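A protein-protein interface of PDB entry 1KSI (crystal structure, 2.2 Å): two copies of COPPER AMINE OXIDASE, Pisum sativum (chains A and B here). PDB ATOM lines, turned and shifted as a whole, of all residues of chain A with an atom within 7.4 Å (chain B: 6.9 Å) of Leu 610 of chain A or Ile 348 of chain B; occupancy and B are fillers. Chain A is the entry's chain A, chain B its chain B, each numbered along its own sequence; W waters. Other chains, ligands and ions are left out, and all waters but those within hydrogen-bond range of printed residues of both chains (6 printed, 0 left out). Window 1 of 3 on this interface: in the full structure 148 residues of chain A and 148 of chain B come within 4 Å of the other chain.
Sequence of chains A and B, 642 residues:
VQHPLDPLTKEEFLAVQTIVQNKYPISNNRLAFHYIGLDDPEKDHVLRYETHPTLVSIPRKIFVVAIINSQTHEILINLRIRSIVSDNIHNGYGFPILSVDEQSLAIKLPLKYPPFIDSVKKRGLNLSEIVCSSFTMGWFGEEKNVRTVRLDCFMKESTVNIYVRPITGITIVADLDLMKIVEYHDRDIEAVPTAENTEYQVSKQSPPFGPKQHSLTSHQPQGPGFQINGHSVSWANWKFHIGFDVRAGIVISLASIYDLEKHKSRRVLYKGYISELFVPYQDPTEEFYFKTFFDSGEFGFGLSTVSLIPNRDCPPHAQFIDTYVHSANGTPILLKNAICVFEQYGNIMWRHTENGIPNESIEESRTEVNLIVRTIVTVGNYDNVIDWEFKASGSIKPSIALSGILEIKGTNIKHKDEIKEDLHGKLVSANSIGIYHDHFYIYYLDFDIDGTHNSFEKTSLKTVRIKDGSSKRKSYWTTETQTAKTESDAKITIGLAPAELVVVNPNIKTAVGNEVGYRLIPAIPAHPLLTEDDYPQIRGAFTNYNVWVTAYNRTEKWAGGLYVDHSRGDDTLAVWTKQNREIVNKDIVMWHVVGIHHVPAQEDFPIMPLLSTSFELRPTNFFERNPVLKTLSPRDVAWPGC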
ATOM      1  N   LEU A 308     -27.138  11.381 -10.214  1.00  0.00           N
ATOM      2  CA  LEU A 308     -25.810  11.456  -9.563  1.00  0.00           C
ATOM      3  C   LEU A 308     -25.160  12.800  -9.830  1.00  0.00           C
ATOM      4  O   LEU A 308     -25.207  13.263 -10.979  1.00  0.00           O
ATOM      5  CB  LEU A 308     -24.942  10.319 -10.070  1.00  0.00           C
ATOM      6  CG  LEU A 308     -25.466   8.916  -9.880  1.00  0.00           C
ATOM      7  CD1 LEU A 308     -24.846   8.011 -10.907  1.00  0.00           C
ATOM      8  CD2 LEU A 308     -25.295   8.408  -8.465  1.00  0.00           C
ATOM      9  N   ARG A 312     -18.718  13.974  -7.970  1.00  0.00           N
ATOM     10  CA  ARG A 312     -18.864  13.859  -6.542  1.00  0.00           C
ATOM     11  C   ARG A 312     -19.402  12.476  -6.290  1.00  0.00           C
ATOM     12  O   ARG A 312     -18.764  11.797  -5.507  1.00  0.00           O
ATOM     13  CB  ARG A 312     -19.802  14.946  -6.018  1.00  0.00           C
ATOM     14  CG  ARG A 312     -19.245  16.343  -6.240  1.00  0.00           C
ATOM     15  CD  ARG A 312     -18.084  16.676  -5.294  1.00  0.00           C
ATOM     16  NE  ARG A 312     -17.701  18.071  -5.439  1.00  0.00           N
ATOM     17  CZ  ARG A 312     -18.308  18.958  -4.593  1.00  0.00           C
ATOM     18  NH1 ARG A 312     -19.212  18.745  -3.618  1.00  0.00           N
ATOM     19  NH2 ARG A 312     -17.993  20.260  -4.761  1.00  0.00           N
ATOM     20  N   ASP A 313     -20.511  12.059  -6.953  1.00  0.00           N
ATOM     21  CA  ASP A 313     -21.010  10.725  -6.626  1.00  0.00           C
ATOM     22  C   ASP A 313     -20.255   9.751  -7.539  1.00  0.00           C
ATOM     23  O   ASP A 313     -20.316   8.568  -7.291  1.00  0.00           O
ATOM     24  CB  ASP A 313     -22.510  10.575  -6.850  1.00  0.00           C
ATOM     25  CG  ASP A 313     -23.359  11.367  -5.887  1.00  0.00           C
ATOM     26  OD1 ASP A 313     -23.136  11.404  -4.657  1.00  0.00           O
ATOM     27  OD2 ASP A 313     -24.346  12.021  -6.358  1.00  0.00           O
ATOM     28  N   CYS A 314     -19.656  10.253  -8.584  1.00  0.00           N
ATOM     29  CA  CYS A 314     -18.902   9.448  -9.531  1.00  0.00           C
ATOM     30  C   CYS A 314     -17.674  10.275  -9.887  1.00  0.00           C
ATOM     31  O   CYS A 314     -17.803  11.501  -9.895  1.00  0.00           O
ATOM     32  CB  CYS A 314     -19.716   9.188 -10.815  1.00  0.00           C
ATOM     33  SG  CYS A 314     -21.192   8.236 -10.394  1.00  0.00           S
ATOM     34  N   ARG A 374     -22.188   2.199 -10.603  1.00  0.00           N
ATOM     35  CA  ARG A 374     -22.801   2.806  -9.415  1.00  0.00           C
ATOM     36  C   ARG A 374     -24.204   3.419  -9.593  1.00  0.00           C
ATOM     37  O   ARG A 374     -24.507   4.064 -10.599  1.00  0.00           O
ATOM     38  CB  ARG A 374     -21.847   3.989  -9.008  1.00  0.00           C
ATOM     39  CG  ARG A 374     -22.463   4.685  -7.792  1.00  0.00           C
ATOM     40  CD  ARG A 374     -21.498   5.666  -7.157  1.00  0.00           C
ATOM     41  NE  ARG A 374     -20.463   4.872  -6.521  1.00  0.00           N
ATOM     42  CZ  ARG A 374     -19.213   5.174  -6.181  1.00  0.00           C
ATOM     43  NH1 ARG A 374     -18.641   6.355  -6.367  1.00  0.00           N
ATOM     44  NH2 ARG A 374     -18.486   4.175  -5.636  1.00  0.00           N
ATOM     45  N   ILE A 376     -27.367   5.519  -6.944  1.00  0.00           N
ATOM     46  CA  ILE A 376     -27.734   5.913  -5.570  1.00  0.00           C
ATOM     47  C   ILE A 376     -29.254   6.025  -5.380  1.00  0.00           C
ATOM     48  O   ILE A 376     -29.929   6.659  -6.208  1.00  0.00           O
ATOM     49  CB  ILE A 376     -27.041   7.246  -5.189  1.00  0.00           C
ATOM     50  CG1 ILE A 376     -25.513   7.128  -5.359  1.00  0.00           C
ATOM     51  CG2 ILE A 376     -27.507   7.672  -3.800  1.00  0.00           C
ATOM     52  CD1 ILE A 376     -24.703   8.275  -4.861  1.00  0.00           C
ATOM     53  N   ASP A 383     -29.775   7.495   2.396  1.00  0.00           N
ATOM     54  CA  ASP A 383     -29.118   7.376   1.078  1.00  0.00           C
ATOM     55  C   ASP A 383     -28.340   6.044   0.988  1.00  0.00           C
ATOM     56  O   ASP A 383     -27.665   5.611   1.935  1.00  0.00           O
ATOM     57  CB  ASP A 383     -28.210   8.517   0.788  1.00  0.00           C
ATOM     58  CG  ASP A 383     -28.845   9.869   0.928  1.00  0.00           C
ATOM     59  OD1 ASP A 383     -29.378  10.242   2.002  1.00  0.00           O
ATOM     60  OD2 ASP A 383     -28.769  10.636  -0.062  1.00  0.00           O
ATOM     61  N   VAL A 385     -25.677   3.955  -1.441  1.00  0.00           N
ATOM     62  CA  VAL A 385     -24.804   4.028  -2.619  1.00  0.00           C
ATOM     63  C   VAL A 385     -24.606   2.561  -3.029  1.00  0.00           C
ATOM     64  O   VAL A 385     -24.112   1.820  -2.183  1.00  0.00           O
ATOM     65  CB  VAL A 385     -23.494   4.693  -2.267  1.00  0.00           C
ATOM     66  CG1 VAL A 385     -22.603   4.809  -3.480  1.00  0.00           C
ATOM     67  CG2 VAL A 385     -23.772   6.011  -1.526  1.00  0.00           C
ATOM     68  N   ASP A 387     -23.112  -0.379  -5.453  1.00  0.00           N
ATOM     69  CA  ASP A 387     -22.008  -0.613  -6.384  1.00  0.00           C
ATOM     70  C   ASP A 387     -21.902  -2.070  -6.803  1.00  0.00           C
ATOM     71  O   ASP A 387     -22.084  -2.978  -5.987  1.00  0.00           O
ATOM     72  CB  ASP A 387     -20.618  -0.229  -5.856  1.00  0.00           C
ATOM     73  CG  ASP A 387     -20.392   1.230  -5.599  1.00  0.00           C
ATOM     74  OD1 ASP A 387     -21.047   2.090  -6.213  1.00  0.00           O
ATOM     75  OD2 ASP A 387     -19.553   1.700  -4.785  1.00  0.00           O
ATOM     76  N   ILE A 400     -22.442  -1.913  -0.764  1.00  0.00           N
ATOM     77  CA  ILE A 400     -23.385  -0.929  -0.319  1.00  0.00           C
ATOM     78  C   ILE A 400     -22.780   0.052   0.689  1.00  0.00           C
ATOM     79  O   ILE A 400     -22.208  -0.374   1.714  1.00  0.00           O
ATOM     80  CB  ILE A 400     -24.599  -1.614   0.359  1.00  0.00           C
ATOM     81  CG1 ILE A 400     -25.424  -2.469  -0.634  1.00  0.00           C
ATOM     82  CG2 ILE A 400     -25.563  -0.618   1.012  1.00  0.00           C
ATOM     83  CD1 ILE A 400     -25.988  -3.611   0.202  1.00  0.00           C
ATOM     84  N   ALA A 401     -22.919   1.356   0.440  1.00  0.00           N
ATOM     85  CA  ALA A 401     -22.527   2.338   1.454  1.00  0.00           C
ATOM     86  C   ALA A 401     -23.751   3.112   1.956  1.00  0.00           C
ATOM     87  O   ALA A 401     -24.639   3.482   1.169  1.00  0.00           O
ATOM     88  CB  ALA A 401     -21.492   3.222   0.795  1.00  0.00           C
ATOM     89  N   LEU A 402     -23.890   3.435   3.235  1.00  0.00           N
ATOM     90  CA  LEU A 402     -24.951   4.189   3.859  1.00  0.00           C
ATOM     91  C   LEU A 402     -24.550   5.610   4.196  1.00  0.00           C
ATOM     92  O   LEU A 402     -23.464   5.785   4.788  1.00  0.00           O
ATOM     93  CB  LEU A 402     -25.371   3.534   5.183  1.00  0.00           C
ATOM     94  CG  LEU A 402     -25.687   2.042   5.225  1.00  0.00           C
ATOM     95  CD1 LEU A 402     -26.540   1.586   6.397  1.00  0.00           C
ATOM     96  CD2 LEU A 402     -26.399   1.571   3.970  1.00  0.00           C
ATOM     97  N   SER A 403     -25.301   6.618   3.812  1.00  0.00           N
ATOM     98  CA  SER A 403     -25.121   8.007   4.226  1.00  0.00           C
ATOM     99  C   SER A 403     -26.518   8.636   4.533  1.00  0.00           C
ATOM    100  O   SER A 403     -27.464   7.869   4.782  1.00  0.00           O
ATOM    101  CB  SER A 403     -24.342   8.864   3.247  1.00  0.00           C
ATOM    102  OG  SER A 403     -24.063  10.130   3.888  1.00  0.00           O
ATOM    103  N   GLY A 404     -26.739   9.959   4.561  1.00  0.00           N
ATOM    104  CA  GLY A 404     -28.011  10.498   4.920  1.00  0.00           C
ATOM    105  C   GLY A 404     -28.114  10.973   6.367  1.00  0.00           C
ATOM    106  O   GLY A 404     -27.151  11.389   7.010  1.00  0.00           O
ATOM    107  N   ILE A 607     -25.549  14.859   9.745  1.00  0.00           N
ATOM    108  CA  ILE A 607     -25.528  14.012   8.561  1.00  0.00           C
ATOM    109  C   ILE A 607     -24.405  12.946   8.742  1.00  0.00           C
ATOM    110  O   ILE A 607     -23.373  13.155   9.422  1.00  0.00           O
ATOM    111  CB  ILE A 607     -25.388  14.850   7.301  1.00  0.00           C
ATOM    112  CG1 ILE A 607     -25.690  14.067   6.024  1.00  0.00           C
ATOM    113  CG2 ILE A 607     -24.076  15.642   7.261  1.00  0.00           C
ATOM    114  CD1 ILE A 607     -25.940  14.982   4.827  1.00  0.00           C
ATOM    115  N   MET A 608     -24.534  11.781   8.121  1.00  0.00           N
ATOM    116  CA  MET A 608     -23.632  10.706   8.492  1.00  0.00           C
ATOM    117  C   MET A 608     -22.515  10.330   7.550  1.00  0.00           C
ATOM    118  O   MET A 608     -22.651  10.149   6.342  1.00  0.00           O
ATOM    119  CB  MET A 608     -24.557   9.599   8.913  1.00  0.00           C
ATOM    120  CG  MET A 608     -24.354   8.333   8.165  1.00  0.00           C
ATOM    121  SD  MET A 608     -25.297   7.027   8.981  1.00  0.00           S
ATOM    122  CE  MET A 608     -24.391   5.599   8.339  1.00  0.00           C
ATOM    123  N   PRO A 609     -21.304  10.204   8.165  1.00  0.00           N
ATOM    124  CA  PRO A 609     -20.114   9.760   7.410  1.00  0.00           C
ATOM    125  C   PRO A 609     -20.401   8.382   6.823  1.00  0.00           C
ATOM    126  O   PRO A 609     -21.023   7.496   7.475  1.00  0.00           O
ATOM    127  CB  PRO A 609     -18.958   9.879   8.389  1.00  0.00           C
ATOM    128  CG  PRO A 609     -19.426  10.585   9.622  1.00  0.00           C
ATOM    129  CD  PRO A 609     -20.924  10.714   9.492  1.00  0.00           C
ATOM    130  N   LEU A 610     -20.046   8.227   5.561  1.00  0.00           N
ATOM    131  CA  LEU A 610     -20.282   6.941   4.924  1.00  0.00           C
ATOM    132  C   LEU A 610     -19.872   5.742   5.781  1.00  0.00           C
ATOM    133  O   LEU A 610     -18.838   5.707   6.474  1.00  0.00           O
ATOM    134  CB  LEU A 610     -19.503   6.878   3.609  1.00  0.00           C
ATOM    135  CG  LEU A 610     -20.208   6.260   2.398  1.00  0.00           C
ATOM    136  CD1 LEU A 610     -21.213   7.314   1.909  1.00  0.00           C
ATOM    137  CD2 LEU A 610     -19.289   5.970   1.235  1.00  0.00           C
ATOM    138  N   LEU A 611     -20.663   4.688   5.801  1.00  0.00           N
ATOM    139  CA  LEU A 611     -20.491   3.453   6.421  1.00  0.00           C
ATOM    140  C   LEU A 611     -20.761   2.419   5.302  1.00  0.00           C
ATOM    141  O   LEU A 611     -21.792   2.406   4.665  1.00  0.00           O
ATOM    142  CB  LEU A 611     -21.401   3.119   7.558  1.00  0.00           C
ATOM    143  CG  LEU A 611     -20.962   1.777   8.198  1.00  0.00           C
ATOM    144  CD1 LEU A 611     -19.910   2.069   9.264  1.00  0.00           C
ATOM    145  CD2 LEU A 611     -22.146   1.118   8.863  1.00  0.00           C
ATOM    146  N   SER A 612     -19.812   1.521   5.133  1.00  0.00           N
ATOM    147  CA  SER A 612     -19.750   0.663   3.956  1.00  0.00           C
ATOM    148  C   SER A 612     -19.649  -0.821   4.245  1.00  0.00           C
ATOM    149  O   SER A 612     -19.282  -1.268   5.330  1.00  0.00           O
ATOM    150  CB  SER A 612     -18.455   1.192   3.324  1.00  0.00           C
ATOM    151  OG  SER A 612     -18.370   0.735   2.029  1.00  0.00           O
ATOM    152  N   GLY B 346     -11.452   9.792  -4.779  1.00  0.00           N
ATOM    153  CA  GLY B 346     -12.667   9.309  -5.439  1.00  0.00           C
ATOM    154  C   GLY B 346     -13.736   8.770  -4.559  1.00  0.00           C
ATOM    155  O   GLY B 346     -14.788   8.408  -5.124  1.00  0.00           O
ATOM    156  N   ASN B 347     -13.563   8.702  -3.257  1.00  0.00           N
ATOM    157  CA  ASN B 347     -14.577   8.173  -2.373  1.00  0.00           C
ATOM    158  C   ASN B 347     -15.583   9.237  -1.909  1.00  0.00           C
ATOM    159  O   ASN B 347     -15.118  10.360  -1.695  1.00  0.00           O
ATOM    160  CB  ASN B 347     -13.862   7.740  -1.070  1.00  0.00           C
ATOM    161  CG  ASN B 347     -13.451   6.295  -1.184  1.00  0.00           C
ATOM    162  OD1 ASN B 347     -13.055   5.832  -2.248  1.00  0.00           O
ATOM    163  ND2 ASN B 347     -13.573   5.558  -0.094  1.00  0.00           N
ATOM    164  N   ILE B 348     -16.823   8.857  -1.701  1.00  0.00           N
ATOM    165  CA  ILE B 348     -17.818   9.840  -1.260  1.00  0.00           C
ATOM    166  C   ILE B 348     -17.589   9.959   0.227  1.00  0.00           C
ATOM    167  O   ILE B 348     -17.519   8.929   0.911  1.00  0.00           O
ATOM    168  CB  ILE B 348     -19.253   9.324  -1.579  1.00  0.00           C
ATOM    169  CG1 ILE B 348     -19.486   9.211  -3.105  1.00  0.00           C
ATOM    170  CG2 ILE B 348     -20.354  10.117  -0.871  1.00  0.00           C
ATOM    171  CD1 ILE B 348     -20.671   8.260  -3.396  1.00  0.00           C
ATOM    172  N   MET B 349     -17.482  11.149   0.770  1.00  0.00           N
ATOM    173  CA  MET B 349     -17.307  11.316   2.223  1.00  0.00           C
ATOM    174  C   MET B 349     -18.611  11.209   2.989  1.00  0.00           C
ATOM    175  O   MET B 349     -18.777  10.567   4.064  1.00  0.00           O
ATOM    176  CB  MET B 349     -16.552  12.637   2.351  1.00  0.00           C
ATOM    177  CG  MET B 349     -16.273  13.058   3.781  1.00  0.00           C
ATOM    178  SD  MET B 349     -15.237  14.505   3.820  1.00  0.00           S
ATOM    179  CE  MET B 349     -15.952  15.749   2.793  1.00  0.00           C
ATOM    180  N   TRP B 350     -19.642  11.887   2.442  1.00  0.00           N
ATOM    181  CA  TRP B 350     -21.030  11.851   2.881  1.00  0.00           C
ATOM    182  C   TRP B 350     -21.910  12.536   1.794  1.00  0.00           C
ATOM    183  O   TRP B 350     -21.461  13.273   0.869  1.00  0.00           O
ATOM    184  CB  TRP B 350     -21.299  12.407   4.276  1.00  0.00           C
ATOM    185  CG  TRP B 350     -20.829  13.777   4.580  1.00  0.00           C
ATOM    186  CD1 TRP B 350     -19.675  14.089   5.244  1.00  0.00           C
ATOM    187  CD2 TRP B 350     -21.435  15.063   4.289  1.00  0.00           C
ATOM    188  NE1 TRP B 350     -19.546  15.452   5.407  1.00  0.00           N
ATOM    189  CE2 TRP B 350     -20.610  16.068   4.813  1.00  0.00           C
ATOM    190  CE3 TRP B 350     -22.611  15.453   3.634  1.00  0.00           C
ATOM    191  CZ2 TRP B 350     -20.895  17.432   4.708  1.00  0.00           C
ATOM    192  CZ3 TRP B 350     -22.914  16.798   3.539  1.00  0.00           C
ATOM    193  CH2 TRP B 350     -22.069  17.778   4.058  1.00  0.00           C
ATOM    194  N   ARG B 351     -23.210  12.265   1.870  1.00  0.00           N
ATOM    195  CA  ARG B 351     -24.130  12.904   0.905  1.00  0.00           C
ATOM    196  C   ARG B 351     -25.597  12.846   1.346  1.00  0.00           C
ATOM    197  O   ARG B 351     -26.009  12.075   2.269  1.00  0.00           O
ATOM    198  CB  ARG B 351     -23.965  12.216  -0.491  1.00  0.00           C
ATOM    199  CG  ARG B 351     -24.742  10.910  -0.530  1.00  0.00           C
ATOM    200  CD  ARG B 351     -24.945  10.214  -1.826  1.00  0.00           C
ATOM    201  NE  ARG B 351     -25.201  11.100  -2.952  1.00  0.00           N
ATOM    202  CZ  ARG B 351     -26.382  11.696  -3.315  1.00  0.00           C
ATOM    203  NH1 ARG B 351     -27.464  11.479  -2.565  1.00  0.00           N
ATOM    204  NH2 ARG B 351     -26.378  12.482  -4.412  1.00  0.00           N
ATOM    205  N   GLU B 364     -26.668  17.333  -1.744  1.00  0.00           N
ATOM    206  CA  GLU B 364     -25.266  17.593  -1.378  1.00  0.00           C
ATOM    207  C   GLU B 364     -24.473  16.284  -1.399  1.00  0.00           C
ATOM    208  O   GLU B 364     -24.876  15.299  -0.755  1.00  0.00           O
ATOM    209  CB  GLU B 364     -25.234  18.241   0.019  1.00  0.00           C
ATOM    210  CG  GLU B 364     -23.892  18.627   0.599  1.00  0.00           C
ATOM    211  CD  GLU B 364     -23.371  19.939   0.115  1.00  0.00           C
ATOM    212  OE1 GLU B 364     -24.087  20.634  -0.616  1.00  0.00           O
ATOM    213  OE2 GLU B 364     -22.263  20.421   0.415  1.00  0.00           O
ATOM    214  N   SER B 365     -23.386  16.323  -2.138  1.00  0.00           N
ATOM    215  CA  SER B 365     -22.430  15.194  -2.122  1.00  0.00           C
ATOM    216  C   SER B 365     -20.998  15.684  -1.917  1.00  0.00           C
ATOM    217  O   SER B 365     -20.539  16.558  -2.693  1.00  0.00           O
ATOM    218  CB  SER B 365     -22.435  14.425  -3.438  1.00  0.00           C
ATOM    219  OG  SER B 365     -21.997  13.118  -3.171  1.00  0.00           O
ATOM    220  N   ARG B 366     -20.296  15.203  -0.908  1.00  0.00           N
ATOM    221  CA  ARG B 366     -18.879  15.689  -0.802  1.00  0.00           C
ATOM    222  C   ARG B 366     -17.943  14.478  -0.882  1.00  0.00           C
ATOM    223  O   ARG B 366     -18.289  13.373  -0.476  1.00  0.00           O
ATOM    224  CB  ARG B 366     -18.654  16.482   0.469  1.00  0.00           C
ATOM    225  CG  ARG B 366     -19.633  17.566   0.849  1.00  0.00           C
ATOM    226  CD  ARG B 366     -18.973  18.768   1.484  1.00  0.00           C
ATOM    227  NE  ARG B 366     -19.922  19.708   2.030  1.00  0.00           N
ATOM    228  CZ  ARG B 366     -19.908  20.435   3.120  1.00  0.00           C
ATOM    229  NH1 ARG B 366     -18.885  20.418   3.987  1.00  0.00           N
ATOM    230  NH2 ARG B 366     -20.965  21.218   3.410  1.00  0.00           N
ATOM    231  N   THR B 367     -16.751  14.649  -1.429  1.00  0.00           N
ATOM    232  CA  THR B 367     -15.784  13.537  -1.469  1.00  0.00           C
ATOM    233  C   THR B 367     -14.596  13.745  -0.518  1.00  0.00           C
ATOM    234  O   THR B 367     -14.253  14.853  -0.080  1.00  0.00           O
ATOM    235  CB  THR B 367     -15.346  13.285  -2.909  1.00  0.00           C
ATOM    236  OG1 THR B 367     -14.872  14.521  -3.448  1.00  0.00           O
ATOM    237  CG2 THR B 367     -16.452  12.762  -3.844  1.00  0.00           C
ATOM    238  N   GLU B 368     -13.943  12.662  -0.133  1.00  0.00           N
ATOM    239  CA  GLU B 368     -12.779  12.636   0.757  1.00  0.00           C
ATOM    240  C   GLU B 368     -11.531  12.184   0.037  1.00  0.00           C
ATOM    241  O   GLU B 368     -11.564  11.371  -0.918  1.00  0.00           O
ATOM    242  CB  GLU B 368     -13.070  11.676   1.912  1.00  0.00           C
ATOM    243  CG  GLU B 368     -13.155  10.206   1.403  1.00  0.00           C
ATOM    244  CD  GLU B 368     -13.678   9.397   2.563  1.00  0.00           C
ATOM    245  OE1 GLU B 368     -14.083   9.983   3.604  1.00  0.00           O
ATOM    246  OE2 GLU B 368     -13.757   8.155   2.537  1.00  0.00           O
ATOM    247  N   LYS B 391      -8.255   8.593   7.726  1.00  0.00           N
ATOM    248  CA  LYS B 391      -9.275   9.487   7.082  1.00  0.00           C
ATOM    249  C   LYS B 391      -9.527  10.779   7.854  1.00  0.00           C
ATOM    250  O   LYS B 391      -9.417  10.837   9.100  1.00  0.00           O
ATOM    251  CB  LYS B 391     -10.611   8.756   6.932  1.00  0.00           C
ATOM    252  CG  LYS B 391     -10.403   7.485   6.103  1.00  0.00           C
ATOM    253  CD  LYS B 391     -11.617   6.563   6.217  1.00  0.00           C
ATOM    254  CE  LYS B 391     -12.555   6.845   5.047  1.00  0.00           C
ATOM    255  NZ  LYS B 391     -13.980   6.529   5.285  1.00  0.00           N
ATOM    256  N   SER B 393     -12.213  12.006   8.593  1.00  0.00           N
ATOM    257  CA  SER B 393     -13.305  11.710   9.484  1.00  0.00           C
ATOM    258  C   SER B 393     -12.881  11.078  10.784  1.00  0.00           C
ATOM    259  O   SER B 393     -13.762  10.771  11.605  1.00  0.00           O
ATOM    260  CB  SER B 393     -14.327  10.769   8.816  1.00  0.00           C
ATOM    261  OG  SER B 393     -13.758   9.492   8.559  1.00  0.00           O
ATOM    262  N   SER B 395     -11.373   8.031  11.127  1.00  0.00           N
ATOM    263  CA  SER B 395     -11.278   6.584  11.039  1.00  0.00           C
ATOM    264  C   SER B 395      -9.849   6.153  10.584  1.00  0.00           C
ATOM    265  O   SER B 395      -9.191   6.765   9.710  1.00  0.00           O
ATOM    266  CB  SER B 395     -12.269   6.022  10.017  1.00  0.00           C
ATOM    267  OG  SER B 395     -13.544   5.688  10.557  1.00  0.00           O
ATOM    268  N   GLU B 616     -11.838  -1.565  10.868  1.00  0.00           N
ATOM    269  CA  GLU B 616     -11.870  -0.085  10.960  1.00  0.00           C
ATOM    270  C   GLU B 616     -11.914   0.321  12.415  1.00  0.00           C
ATOM    271  O   GLU B 616     -12.503  -0.433  13.186  1.00  0.00           O
ATOM    272  CB  GLU B 616     -13.071   0.450  10.183  1.00  0.00           C
ATOM    273  CG  GLU B 616     -13.331   1.939  10.409  1.00  0.00           C
ATOM    274  CD  GLU B 616     -14.519   2.492   9.584  1.00  0.00           C
ATOM    275  OE1 GLU B 616     -15.260   1.749   8.914  1.00  0.00           O
ATOM    276  OE2 GLU B 616     -14.766   3.706   9.666  1.00  0.00           O
ATOM    277  N   ARG B 618     -13.201   3.291  14.381  1.00  0.00           N
ATOM    278  CA  ARG B 618     -14.135   4.410  14.118  1.00  0.00           C
ATOM    279  C   ARG B 618     -14.464   5.259  15.331  1.00  0.00           C
ATOM    280  O   ARG B 618     -14.875   4.747  16.362  1.00  0.00           O
ATOM    281  CB  ARG B 618     -15.406   3.742  13.538  1.00  0.00           C
ATOM    282  CG  ARG B 618     -16.499   4.659  13.016  1.00  0.00           C
ATOM    283  CD  ARG B 618     -17.032   4.146  11.707  1.00  0.00           C
ATOM    284  NE  ARG B 618     -18.149   4.983  11.233  1.00  0.00           N
ATOM    285  CZ  ARG B 618     -18.347   5.336   9.963  1.00  0.00           C
ATOM    286  NH1 ARG B 618     -17.468   4.920   9.058  1.00  0.00           N
ATOM    287  NH2 ARG B 618     -19.397   6.086   9.604  1.00  0.00           N
HETATM  288  O   HOH W   1     -16.609   7.273   6.805  1.00  0.00           O
HETATM  289  O   HOH W   2     -20.671  20.837  -1.866  1.00  0.00           O
HETATM  290  O   HOH W   3     -15.849   6.100  -5.350  1.00  0.00           O
HETATM  291  O   HOH W   4     -16.456  10.187  -6.427  1.00  0.00           O
HETATM  292  O   HOH W   5     -22.116   5.759  10.310  1.00  0.00           O
HETATM  293  O   HOH W   6     -17.000   2.031   6.605  1.00  0.00           O
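The backbone carbonyl oxygen (O) of Ser 365 of chain B is in hydrogen-bond range of the guanidinium group (NH1) of Arg 312 of chain A. The side-chain hydroxyl (OG) of Ser 403 of chain A sits at hydrogen-bond distance from the backbone NH (N) of Arg 351 of chain B (3.1 Å). OD1 of Asp 313 of chain A lies within hydrogen-bond range of OG of Ser 365 of chain B, 2.5 Å away. The backbone NH (N) of Gly 404 of chain A is in hydrogen-bond range of the backbone carbonyl oxygen (O) of Arg 351 of chain B. The backbone carbonyl oxygen (O) of Leu 610 of chain A lies within hydrogen-bond range of the guanidinium group (NH1) of Arg 618 of chain B (3.0 Å). The guanidinium group (NE) of Arg 351 of chain B is in salt-bridge range of the side-chain carboxylate (OD1) of Asp 313 of chain A. NH1 of Arg 351 of chain B is in salt-bridge range of OD2 of Asp 383 of chain A. O of Met 349 of chain B sits at hydrogen-bond distance from N of Leu 610 of chain A, at 3.1 Å. O of Pro 609 of chain A sits at hydrogen-bond distance from NH2 of Arg 618 of chain B, 3.0 Å away.
The side-chain carboxylate (OE2) of Glu 616 of chain B is in salt-bridge range of the guanidinium group (NH1) of Arg 618 of chain B.
Of chain B, only Ile 348, Met 349 and Arg 618 come within 4 Å of Leu 610 of chain A. Printed residues of chain B within 4 Å of Leu 611 of chain A: Arg 618 (3.7 Å). Ile 348 of chain B touches four residues of chain A. Printed residues of chain A within 4 Å of Trp 350 of chain B: Ser 403 (3.6 Å), Ile 607 (3.6 Å) and Met 608 (3.3 Å). The nearest residue of chain B that does not touch Leu 610 of chain A is Trp 350 of chain B (4.5 Å). The nearest printed residue of chain B that does not touch Asp 313 of chain A is Thr 367 of chain B (5.2 Å).
Of the 20 printed residues of chain A, 12 touch a printed residue of chain B. Hydrophobic or aromatic side chains of chain A that line the printed part of chain B: Ile 376, Val 385, Ile 607, Leu 610 and Leu 611. Along chain A the printed residues that touch a printed residue of chain B span positions 312 to 611. Among the printed residues, Asp or Glu carboxylates within 4 Å of a Lys or Arg side-chain nitrogen of the other chain: Asp 313 of chain A with Arg 351 of chain B and Asp 383 of chain A with Arg 351 of chain B.
No position is printed for both chains. Of the 21 pairs that touch across the chains among the printed residues, none has its exchanged pair printed and touching as well.
Water W3 bridges O of Gly 346 of chain B and NH1 of Arg 374 of chain A. Water W5 lies within hydrogen-bond range of NH2 of Arg 618 of chain B, O of Pro 609 of chain A and SD of Met 608 of chain A.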
